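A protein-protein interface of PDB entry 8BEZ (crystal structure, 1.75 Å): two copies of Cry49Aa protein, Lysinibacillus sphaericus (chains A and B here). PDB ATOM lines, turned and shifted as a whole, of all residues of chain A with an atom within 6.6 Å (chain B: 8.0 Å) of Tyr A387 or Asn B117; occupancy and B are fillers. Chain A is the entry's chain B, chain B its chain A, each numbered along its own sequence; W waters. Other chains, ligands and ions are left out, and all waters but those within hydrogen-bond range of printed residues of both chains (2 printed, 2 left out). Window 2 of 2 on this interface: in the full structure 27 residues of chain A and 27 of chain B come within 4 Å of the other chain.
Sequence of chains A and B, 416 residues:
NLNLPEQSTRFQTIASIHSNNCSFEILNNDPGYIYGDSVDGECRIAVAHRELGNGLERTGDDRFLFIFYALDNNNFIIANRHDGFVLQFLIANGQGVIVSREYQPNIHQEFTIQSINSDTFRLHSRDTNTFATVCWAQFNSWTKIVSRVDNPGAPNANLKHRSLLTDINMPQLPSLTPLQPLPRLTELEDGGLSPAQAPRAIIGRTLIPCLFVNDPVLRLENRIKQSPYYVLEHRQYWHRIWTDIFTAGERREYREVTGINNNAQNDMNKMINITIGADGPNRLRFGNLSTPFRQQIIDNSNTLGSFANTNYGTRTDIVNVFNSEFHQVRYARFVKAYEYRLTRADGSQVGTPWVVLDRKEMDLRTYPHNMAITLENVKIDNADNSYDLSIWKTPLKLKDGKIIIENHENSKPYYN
N of Ser B115 lies within hydrogen-bond range of O of Phe A307, 2.8 Å away.
O of Asn B117 lies within hydrogen-bond range of OH of Tyr A387, at 3.4 Å.
The side-chain hydroxyl (OG) of Ser B118 is in hydrogen-bond range of the backbone carbonyl oxygen (O) of Tyr A387 (3.1 Å).
OG of Ser B118 lies close to OD2 of Asp A388, 3.1 Å away.
The backbone NH (N) of Arg B122 lies within hydrogen-bond range of the backbone carbonyl oxygen (O) of Gln B114.
OD1 of Asn B117 sits close to N of Asp B119.
The side-chain amide oxygen (OD1) of Asn B117 sits at hydrogen-bond distance from the side-chain hydroxyl (OG1) of Thr B120, at 3.0 Å.
The side-chain carboxylate of Asp A279 is in hydrogen-bond range of the backbone NH of Phe A307, 2.8 Å away.
The side-chain amide oxygen (OD1) of Asn A309 lies within hydrogen-bond range of the side-chain hydroxyl (OG1) of Thr A310 (3.2 Å).
OD1 of Asn A385 sits at hydrogen-bond distance from N of Tyr A387 (3.0 Å).
Ile B113 touches Phe A307 (O to CB, 3.6 Å).
Phe A307 touches Gln B114 (O to CA, 3.6 Å).
Ser B115 touches Ala A308 (O to CA, 3.8 Å).
Ser B115 touches Asn A309 (O to OD1, 3.8 Å).
ND2 of Asn A309 touches CD1 of Ile B116, 3.9 Å away.
Ser B115 touches Tyr A387 (CB to OH, 3.2 Å).
CD2 of Tyr A387 touches O of Ile B116, 3.6 Å away.
Ala A278 touches none of the printed residues of chain B.
Printed residues of chain B within 4 Å of Phe A307: Ile B113 (3.6 Å), Gln B114 (3.6 Å) and Ser B115 (2.8 Å).
Printed residues of chain B within 4 Å of Asn A309: Ser B115 and Ile B116.
Asn A385 touches none of the printed residues of chain B.
Tyr A387 touches four residues of chain B.
Printed residues of chain B within 4 Å of Asp A388: Ser B118 (2.9 Å).
Of the printed residues of chain A, Ser B115 touches Phe A307, Ala A308, Asn A309 and Tyr A387.
Printed residues of chain A within 4 Å of Ile B116: Asn A309 and Tyr A387.
The nearest residue of chain B that does not touch Tyr A387 is Thr B120 (5.6 Å).
The nearest printed residue of chain A that does not touch Ser B115 is Asp A279 (4.9 Å).
Printed residues of chain B that touch a printed residue of chain A: Ile B113, Gln B114, Ser B115, Ile B116, Asn B117 and Ser B118.
Hydrophobic or aromatic side chains of chain B that line the printed part of chain A: Ile B116.
Of the 13 printed residues of chain A, 5 touch a printed residue of chain B.
No position is printed for both chains.
Of the 11 pairs that touch across the chains among the printed residues, none has its exchanged pair printed and touching as well.
Water W1 lies within hydrogen-bond range of the side-chain amide nitrogen of Asn B117 (2.7 Å) and the backbone carbonyl oxygen of Ser A386 (2.9 Å).
Water W2 bridges OD2 of Asp A279 and OG of Ser B115.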
ATOM      1  N   ALA A 278      13.649  15.775 -28.904  1.00  0.00           N
ATOM      2  CA  ALA A 278      14.763  15.793 -29.883  1.00  0.00           C
ATOM      3  C   ALA A 278      14.981  14.408 -30.508  1.00  0.00           C
ATOM      4  O   ALA A 278      15.767  14.320 -31.551  1.00  0.00           O
ATOM      5  CB  ALA A 278      16.018  16.302 -29.224  1.00  0.00           C
ATOM      6  N   ASP A 279      14.383  13.342 -29.932  1.00  0.00           N
ATOM      7  CA  ASP A 279      14.642  11.947 -30.397  1.00  0.00           C
ATOM      8  C   ASP A 279      13.823  11.633 -31.662  1.00  0.00           C
ATOM      9  O   ASP A 279      14.131  10.590 -32.344  1.00  0.00           O
ATOM     10  CB  ASP A 279      14.430  10.899 -29.302  1.00  0.00           C
ATOM     11  CG  ASP A 279      13.192  11.007 -28.440  1.00  0.00           C
ATOM     12  OD1 ASP A 279      12.487  12.086 -28.481  1.00  0.00           O
ATOM     13  OD2 ASP A 279      12.966  10.031 -27.668  1.00  0.00           O
ATOM     14  N   GLY A 280      12.873  12.482 -32.054  1.00  0.00           N
ATOM     15  CA  GLY A 280      12.264  12.329 -33.389  1.00  0.00           C
ATOM     16  C   GLY A 280      11.086  13.256 -33.624  1.00  0.00           C
ATOM     17  O   GLY A 280      10.506  13.824 -32.665  1.00  0.00           O
ATOM     18  N   PHE A 307      11.746   9.984 -25.112  1.00  0.00           N
ATOM     19  CA  PHE A 307      12.623   9.651 -23.960  1.00  0.00           C
ATOM     20  C   PHE A 307      13.684  10.741 -23.728  1.00  0.00           C
ATOM     21  O   PHE A 307      14.581  10.543 -22.845  1.00  0.00           O
ATOM     22  CB  PHE A 307      13.292   8.294 -24.182  1.00  0.00           C
ATOM     23  CG  PHE A 307      12.319   7.199 -24.538  1.00  0.00           C
ATOM     24  CD1 PHE A 307      11.161   7.027 -23.806  1.00  0.00           C
ATOM     25  CD2 PHE A 307      12.579   6.327 -25.587  1.00  0.00           C
ATOM     26  CE1 PHE A 307      10.248   6.028 -24.135  1.00  0.00           C
ATOM     27  CE2 PHE A 307      11.677   5.315 -25.898  1.00  0.00           C
ATOM     28  CZ  PHE A 307      10.508   5.180 -25.182  1.00  0.00           C
ATOM     29  N   ALA A 308      13.644  11.822 -24.513  1.00  0.00           N
ATOM     30  CA  ALA A 308      14.664  12.900 -24.480  1.00  0.00           C
ATOM     31  C   ALA A 308      14.318  13.917 -23.383  1.00  0.00           C
ATOM     32  O   ALA A 308      13.127  14.114 -23.085  1.00  0.00           O
ATOM     33  CB  ALA A 308      14.753  13.545 -25.844  1.00  0.00           C
ATOM     34  N   ASN A 309      15.357  14.558 -22.843  1.00  0.00           N
ATOM     35  CA  ASN A 309      15.268  15.668 -21.856  1.00  0.00           C
ATOM     36  C   ASN A 309      15.440  17.015 -22.573  1.00  0.00           C
ATOM     37  O   ASN A 309      15.573  18.047 -21.878  1.00  0.00           O
ATOM     38  CB  ASN A 309      16.327  15.506 -20.753  1.00  0.00           C
ATOM     39  CG  ASN A 309      17.701  15.102 -21.260  1.00  0.00           C
ATOM     40  OD1 ASN A 309      18.134  15.524 -22.330  1.00  0.00           O
ATOM     41  ND2 ASN A 309      18.424  14.300 -20.488  1.00  0.00           N
ATOM     42  N   THR A 310      15.452  16.997 -23.907  1.00  0.00           N
ATOM     43  CA  THR A 310      15.694  18.159 -24.789  1.00  0.00           C
ATOM     44  C   THR A 310      14.596  18.183 -25.855  1.00  0.00           C
ATOM     45  O   THR A 310      14.196  17.066 -26.351  1.00  0.00           O
ATOM     46  CB  THR A 310      17.059  18.017 -25.471  1.00  0.00           C
ATOM     47  OG1 THR A 310      18.072  17.955 -24.472  1.00  0.00           O
ATOM     48  CG2 THR A 310      17.388  19.132 -26.438  1.00  0.00           C
ATOM     49  N   ASN A 311      14.132  19.381 -26.215  1.00  0.00           N
ATOM     50  CA  ASN A 311      13.183  19.577 -27.338  1.00  0.00           C
ATOM     51  C   ASN A 311      13.917  19.588 -28.675  1.00  0.00           C
ATOM     52  O   ASN A 311      15.103  20.048 -28.767  1.00  0.00           O
ATOM     53  CB  ASN A 311      12.379  20.859 -27.169  1.00  0.00           C
ATOM     54  CG  ASN A 311      11.403  20.785 -26.016  1.00  0.00           C
ATOM     55  OD1 ASN A 311      10.864  19.712 -25.652  1.00  0.00           O
ATOM     56  ND2 ASN A 311      11.155  21.947 -25.445  1.00  0.00           N
ATOM     57  N   ASN A 385      21.078  22.407 -30.522  1.00  0.00           N
ATOM     58  CA  ASN A 385      21.524  21.458 -29.461  1.00  0.00           C
ATOM     59  C   ASN A 385      22.444  20.398 -30.079  1.00  0.00           C
ATOM     60  O   ASN A 385      22.607  20.375 -31.343  1.00  0.00           O
ATOM     61  CB  ASN A 385      20.313  20.896 -28.704  1.00  0.00           C
ATOM     62  CG  ASN A 385      19.435  20.022 -29.569  1.00  0.00           C
ATOM     63  OD1 ASN A 385      19.913  19.051 -30.164  1.00  0.00           O
ATOM     64  ND2 ASN A 385      18.159  20.371 -29.694  1.00  0.00           N
ATOM     65  N   SER A 386      23.054  19.579 -29.228  1.00  0.00           N
ATOM     66  CA  SER A 386      24.035  18.549 -29.633  1.00  0.00           C
ATOM     67  C   SER A 386      23.398  17.155 -29.627  1.00  0.00           C
ATOM     68  O   SER A 386      24.172  16.153 -29.536  1.00  0.00           O
ATOM     69  CB  SER A 386      25.283  18.618 -28.751  1.00  0.00           C
ATOM     70  OG  SER A 386      24.933  18.584 -27.377  1.00  0.00           O
ATOM     71  N   TYR A 387      22.069  17.044 -29.675  1.00  0.00           N
ATOM     72  CA  TYR A 387      21.373  15.740 -29.483  1.00  0.00           C
ATOM     73  C   TYR A 387      21.704  14.816 -30.671  1.00  0.00           C
ATOM     74  O   TYR A 387      22.047  13.636 -30.423  1.00  0.00           O
ATOM     75  CB  TYR A 387      19.861  15.908 -29.285  1.00  0.00           C
ATOM     76  CG  TYR A 387      19.170  14.611 -28.936  1.00  0.00           C
ATOM     77  CD1 TYR A 387      18.806  13.702 -29.922  1.00  0.00           C
ATOM     78  CD2 TYR A 387      18.972  14.251 -27.615  1.00  0.00           C
ATOM     79  CE1 TYR A 387      18.239  12.474 -29.605  1.00  0.00           C
ATOM     80  CE2 TYR A 387      18.390  13.032 -27.284  1.00  0.00           C
ATOM     81  CZ  TYR A 387      18.008  12.150 -28.285  1.00  0.00           C
ATOM     82  OH  TYR A 387      17.450  10.946 -27.936  1.00  0.00           O
ATOM     83  N   ASP A 388      21.643  15.337 -31.896  1.00  0.00           N
ATOM     84  CA  ASP A 388      21.832  14.537 -33.143  1.00  0.00           C
ATOM     85  C   ASP A 388      22.739  15.338 -34.078  1.00  0.00           C
ATOM     86  O   ASP A 388      22.276  16.321 -34.717  1.00  0.00           O
ATOM     87  CB  ASP A 388      20.508  14.111 -33.806  1.00  0.00           C
ATOM     88  CG  ASP A 388      20.541  12.747 -34.510  1.00  0.00           C
ATOM     89  OD1 ASP A 388      21.592  12.397 -35.083  1.00  0.00           O
ATOM     90  OD2 ASP A 388      19.492  12.044 -34.484  1.00  0.00           O
ATOM     91  N   LEU A 389      24.010  14.949 -34.114  1.00  0.00           N
ATOM     92  CA  LEU A 389      25.017  15.642 -34.948  1.00  0.00           C
ATOM     93  C   LEU A 389      25.542  14.709 -36.041  1.00  0.00           C
ATOM     94  O   LEU A 389      26.728  14.850 -36.425  1.00  0.00           O
ATOM     95  CB  LEU A 389      26.123  16.149 -34.027  1.00  0.00           C
ATOM     96  CG  LEU A 389      25.666  17.217 -33.035  1.00  0.00           C
ATOM     97  CD1 LEU A 389      26.821  17.678 -32.176  1.00  0.00           C
ATOM     98  CD2 LEU A 389      25.038  18.398 -33.772  1.00  0.00           C
ATOM     99  N   ILE B  17      28.874   2.600 -22.280  1.00  0.00           N
ATOM    100  CA  ILE B  17      29.594   3.176 -23.453  1.00  0.00           C
ATOM    101  C   ILE B  17      31.103   3.147 -23.173  1.00  0.00           C
ATOM    102  O   ILE B  17      31.887   3.322 -24.127  1.00  0.00           O
ATOM    103  CB  ILE B  17      29.104   4.596 -23.796  1.00  0.00           C
ATOM    104  CG1 ILE B  17      29.399   5.607 -22.680  1.00  0.00           C
ATOM    105  CG2 ILE B  17      27.629   4.548 -24.174  1.00  0.00           C
ATOM    106  CD1 ILE B  17      29.356   7.058 -23.133  1.00  0.00           C
ATOM    107  N   ILE B 113      13.633   5.094 -19.515  1.00  0.00           N
ATOM    108  CA  ILE B 113      14.747   5.431 -20.456  1.00  0.00           C
ATOM    109  C   ILE B 113      14.915   6.948 -20.460  1.00  0.00           C
ATOM    110  O   ILE B 113      13.929   7.692 -20.725  1.00  0.00           O
ATOM    111  CB  ILE B 113      14.501   4.879 -21.874  1.00  0.00           C
ATOM    112  CG1 ILE B 113      14.328   3.361 -21.855  1.00  0.00           C
ATOM    113  CG2 ILE B 113      15.605   5.313 -22.838  1.00  0.00           C
ATOM    114  CD1 ILE B 113      13.867   2.788 -23.181  1.00  0.00           C
ATOM    115  N   GLN B 114      16.136   7.409 -20.193  1.00  0.00           N
ATOM    116  CA  GLN B 114      16.491   8.834 -20.286  1.00  0.00           C
ATOM    117  C   GLN B 114      17.534   8.925 -21.405  1.00  0.00           C
ATOM    118  O   GLN B 114      18.707   8.502 -21.178  1.00  0.00           O
ATOM    119  CB  GLN B 114      16.888   9.275 -18.875  1.00  0.00           C
ATOM    120  CG  GLN B 114      17.347  10.715 -18.738  1.00  0.00           C
ATOM    121  CD  GLN B 114      17.895  10.936 -17.346  1.00  0.00           C
ATOM    122  OE1 GLN B 114      19.082  11.216 -17.159  1.00  0.00           O
ATOM    123  NE2 GLN B 114      17.039  10.721 -16.354  1.00  0.00           N
ATOM    124  N   SER B 115      17.116   9.365 -22.592  1.00  0.00           N
ATOM    125  CA  SER B 115      17.993   9.554 -23.772  1.00  0.00           C
ATOM    126  C   SER B 115      18.798  10.843 -23.616  1.00  0.00           C
ATOM    127  O   SER B 115      18.188  11.921 -23.502  1.00  0.00           O
ATOM    128  CB  SER B 115      17.231   9.517 -25.070  1.00  0.00           C
ATOM    129  OG  SER B 115      16.792   8.184 -25.294  1.00  0.00           O
ATOM    130  N   ILE B 116      20.128  10.704 -23.633  1.00  0.00           N
ATOM    131  CA  ILE B 116      21.128  11.815 -23.579  1.00  0.00           C
ATOM    132  C   ILE B 116      21.367  12.334 -25.000  1.00  0.00           C
ATOM    133  O   ILE B 116      21.508  13.581 -25.176  1.00  0.00           O
ATOM    134  CB  ILE B 116      22.438  11.330 -22.914  1.00  0.00           C
ATOM    135  CG1 ILE B 116      22.195  10.873 -21.471  1.00  0.00           C
ATOM    136  CG2 ILE B 116      23.514  12.396 -22.989  1.00  0.00           C
ATOM    137  CD1 ILE B 116      21.436  11.900 -20.630  1.00  0.00           C
ATOM    138  N   ASN B 117      21.443  11.409 -25.956  1.00  0.00           N
ATOM    139  CA  ASN B 117      21.591  11.705 -27.398  1.00  0.00           C
ATOM    140  C   ASN B 117      21.119  10.489 -28.195  1.00  0.00           C
ATOM    141  O   ASN B 117      20.558   9.548 -27.572  1.00  0.00           O
ATOM    142  CB  ASN B 117      23.011  12.176 -27.718  1.00  0.00           C
ATOM    143  CG  ASN B 117      24.067  11.108 -27.549  1.00  0.00           C
ATOM    144  OD1 ASN B 117      23.800   9.915 -27.650  1.00  0.00           O
ATOM    145  ND2 ASN B 117      25.285  11.522 -27.303  1.00  0.00           N
ATOM    146  N   SER B 118      21.307  10.525 -29.518  1.00  0.00           N
ATOM    147  CA  SER B 118      20.756   9.557 -30.505  1.00  0.00           C
ATOM    148  C   SER B 118      21.022   8.104 -30.107  1.00  0.00           C
ATOM    149  O   SER B 118      20.099   7.287 -30.288  1.00  0.00           O
ATOM    150  CB  SER B 118      21.301   9.820 -31.881  1.00  0.00           C
ATOM    151  OG  SER B 118      21.301  11.205 -32.163  1.00  0.00           O
ATOM    152  N   ASP B 119      22.219   7.764 -29.616  1.00  0.00           N
ATOM    153  CA  ASP B 119      22.618   6.343 -29.367  1.00  0.00           C
ATOM    154  C   ASP B 119      23.003   6.098 -27.891  1.00  0.00           C
ATOM    155  O   ASP B 119      23.474   4.969 -27.588  1.00  0.00           O
ATOM    156  CB  ASP B 119      23.754   5.934 -30.317  1.00  0.00           C
ATOM    157  CG  ASP B 119      24.925   6.900 -30.309  1.00  0.00           C
ATOM    158  OD1 ASP B 119      25.280   7.368 -29.206  1.00  0.00           O
ATOM    159  OD2 ASP B 119      25.461   7.213 -31.411  1.00  0.00           O
ATOM    160  N   THR B 120      22.821   7.079 -26.997  1.00  0.00           N
ATOM    161  CA  THR B 120      23.227   7.006 -25.561  1.00  0.00           C
ATOM    162  C   THR B 120      22.020   7.253 -24.652  1.00  0.00           C
ATOM    163  O   THR B 120      21.272   8.256 -24.863  1.00  0.00           O
ATOM    164  CB  THR B 120      24.340   8.003 -25.226  1.00  0.00           C
ATOM    165  OG1 THR B 120      25.342   7.811 -26.222  1.00  0.00           O
ATOM    166  CG2 THR B 120      24.933   7.825 -23.842  1.00  0.00           C
ATOM    167  N   PHE B 121      21.857   6.410 -23.643  1.00  0.00           N
ATOM    168  CA  PHE B 121      20.716   6.488 -22.701  1.00  0.00           C
ATOM    169  C   PHE B 121      21.152   6.054 -21.303  1.00  0.00           C
ATOM    170  O   PHE B 121      22.242   5.418 -21.124  1.00  0.00           O
ATOM    171  CB  PHE B 121      19.536   5.664 -23.228  1.00  0.00           C
ATOM    172  CG  PHE B 121      19.778   4.179 -23.222  1.00  0.00           C
ATOM    173  CD1 PHE B 121      20.339   3.556 -24.320  1.00  0.00           C
ATOM    174  CD2 PHE B 121      19.480   3.408 -22.107  1.00  0.00           C
ATOM    175  CE1 PHE B 121      20.582   2.184 -24.314  1.00  0.00           C
ATOM    176  CE2 PHE B 121      19.739   2.043 -22.093  1.00  0.00           C
ATOM    177  CZ  PHE B 121      20.290   1.433 -23.199  1.00  0.00           C
ATOM    178  N   ARG B 122      20.309   6.380 -20.326  1.00  0.00           N
ATOM    179  CA  ARG B 122      20.440   5.933 -18.921  1.00  0.00           C
ATOM    180  C   ARG B 122      19.190   5.144 -18.538  1.00  0.00           C
ATOM    181  O   ARG B 122      18.078   5.436 -19.107  1.00  0.00           O
ATOM    182  CB  ARG B 122      20.674   7.146 -18.024  1.00  0.00           C
ATOM    183  CG  ARG B 122      21.844   8.006 -18.477  1.00  0.00           C
ATOM    184  CD  ARG B 122      21.844   9.353 -17.784  1.00  0.00           C
ATOM    185  NE  ARG B 122      22.571   9.254 -16.536  1.00  0.00           N
ATOM    186  CZ  ARG B 122      22.384  10.002 -15.449  1.00  0.00           C
ATOM    187  NH1 ARG B 122      21.436  10.920 -15.404  1.00  0.00           N
ATOM    188  NH2 ARG B 122      23.165   9.815 -14.396  1.00  0.00           N
ATOM    189  N   ASN B 158      26.082   6.202 -18.423  1.00  0.00           N
ATOM    190  CA  ASN B 158      25.729   6.287 -19.866  1.00  0.00           C
ATOM    191  C   ASN B 158      25.854   4.891 -20.475  1.00  0.00           C
ATOM    192  O   ASN B 158      26.943   4.255 -20.352  1.00  0.00           O
ATOM    193  CB  ASN B 158      26.562   7.336 -20.609  1.00  0.00           C
ATOM    194  CG  ASN B 158      26.263   8.748 -20.156  1.00  0.00           C
ATOM    195  OD1 ASN B 158      25.316   8.987 -19.419  1.00  0.00           O
ATOM    196  ND2 ASN B 158      27.048   9.694 -20.610  1.00  0.00           N
ATOM    197  N   LEU B 159      24.768   4.424 -21.096  1.00  0.00           N
ATOM    198  CA  LEU B 159      24.649   3.077 -21.691  1.00  0.00           C
ATOM    199  C   LEU B 159      24.380   3.182 -23.193  1.00  0.00           C
ATOM    200  O   LEU B 159      23.973   4.281 -23.684  1.00  0.00           O
ATOM    201  CB  LEU B 159      23.506   2.321 -21.013  1.00  0.00           C
ATOM    202  CG  LEU B 159      23.561   2.239 -19.489  1.00  0.00           C
ATOM    203  CD1 LEU B 159      22.313   1.579 -18.949  1.00  0.00           C
ATOM    204  CD2 LEU B 159      24.807   1.492 -19.014  1.00  0.00           C
HETATM  205  O   HOH W   1      25.430  14.183 -27.800  1.00  0.00           O
HETATM  206  O   HOH W   2      14.955   8.144 -27.520  1.00  0.00           O
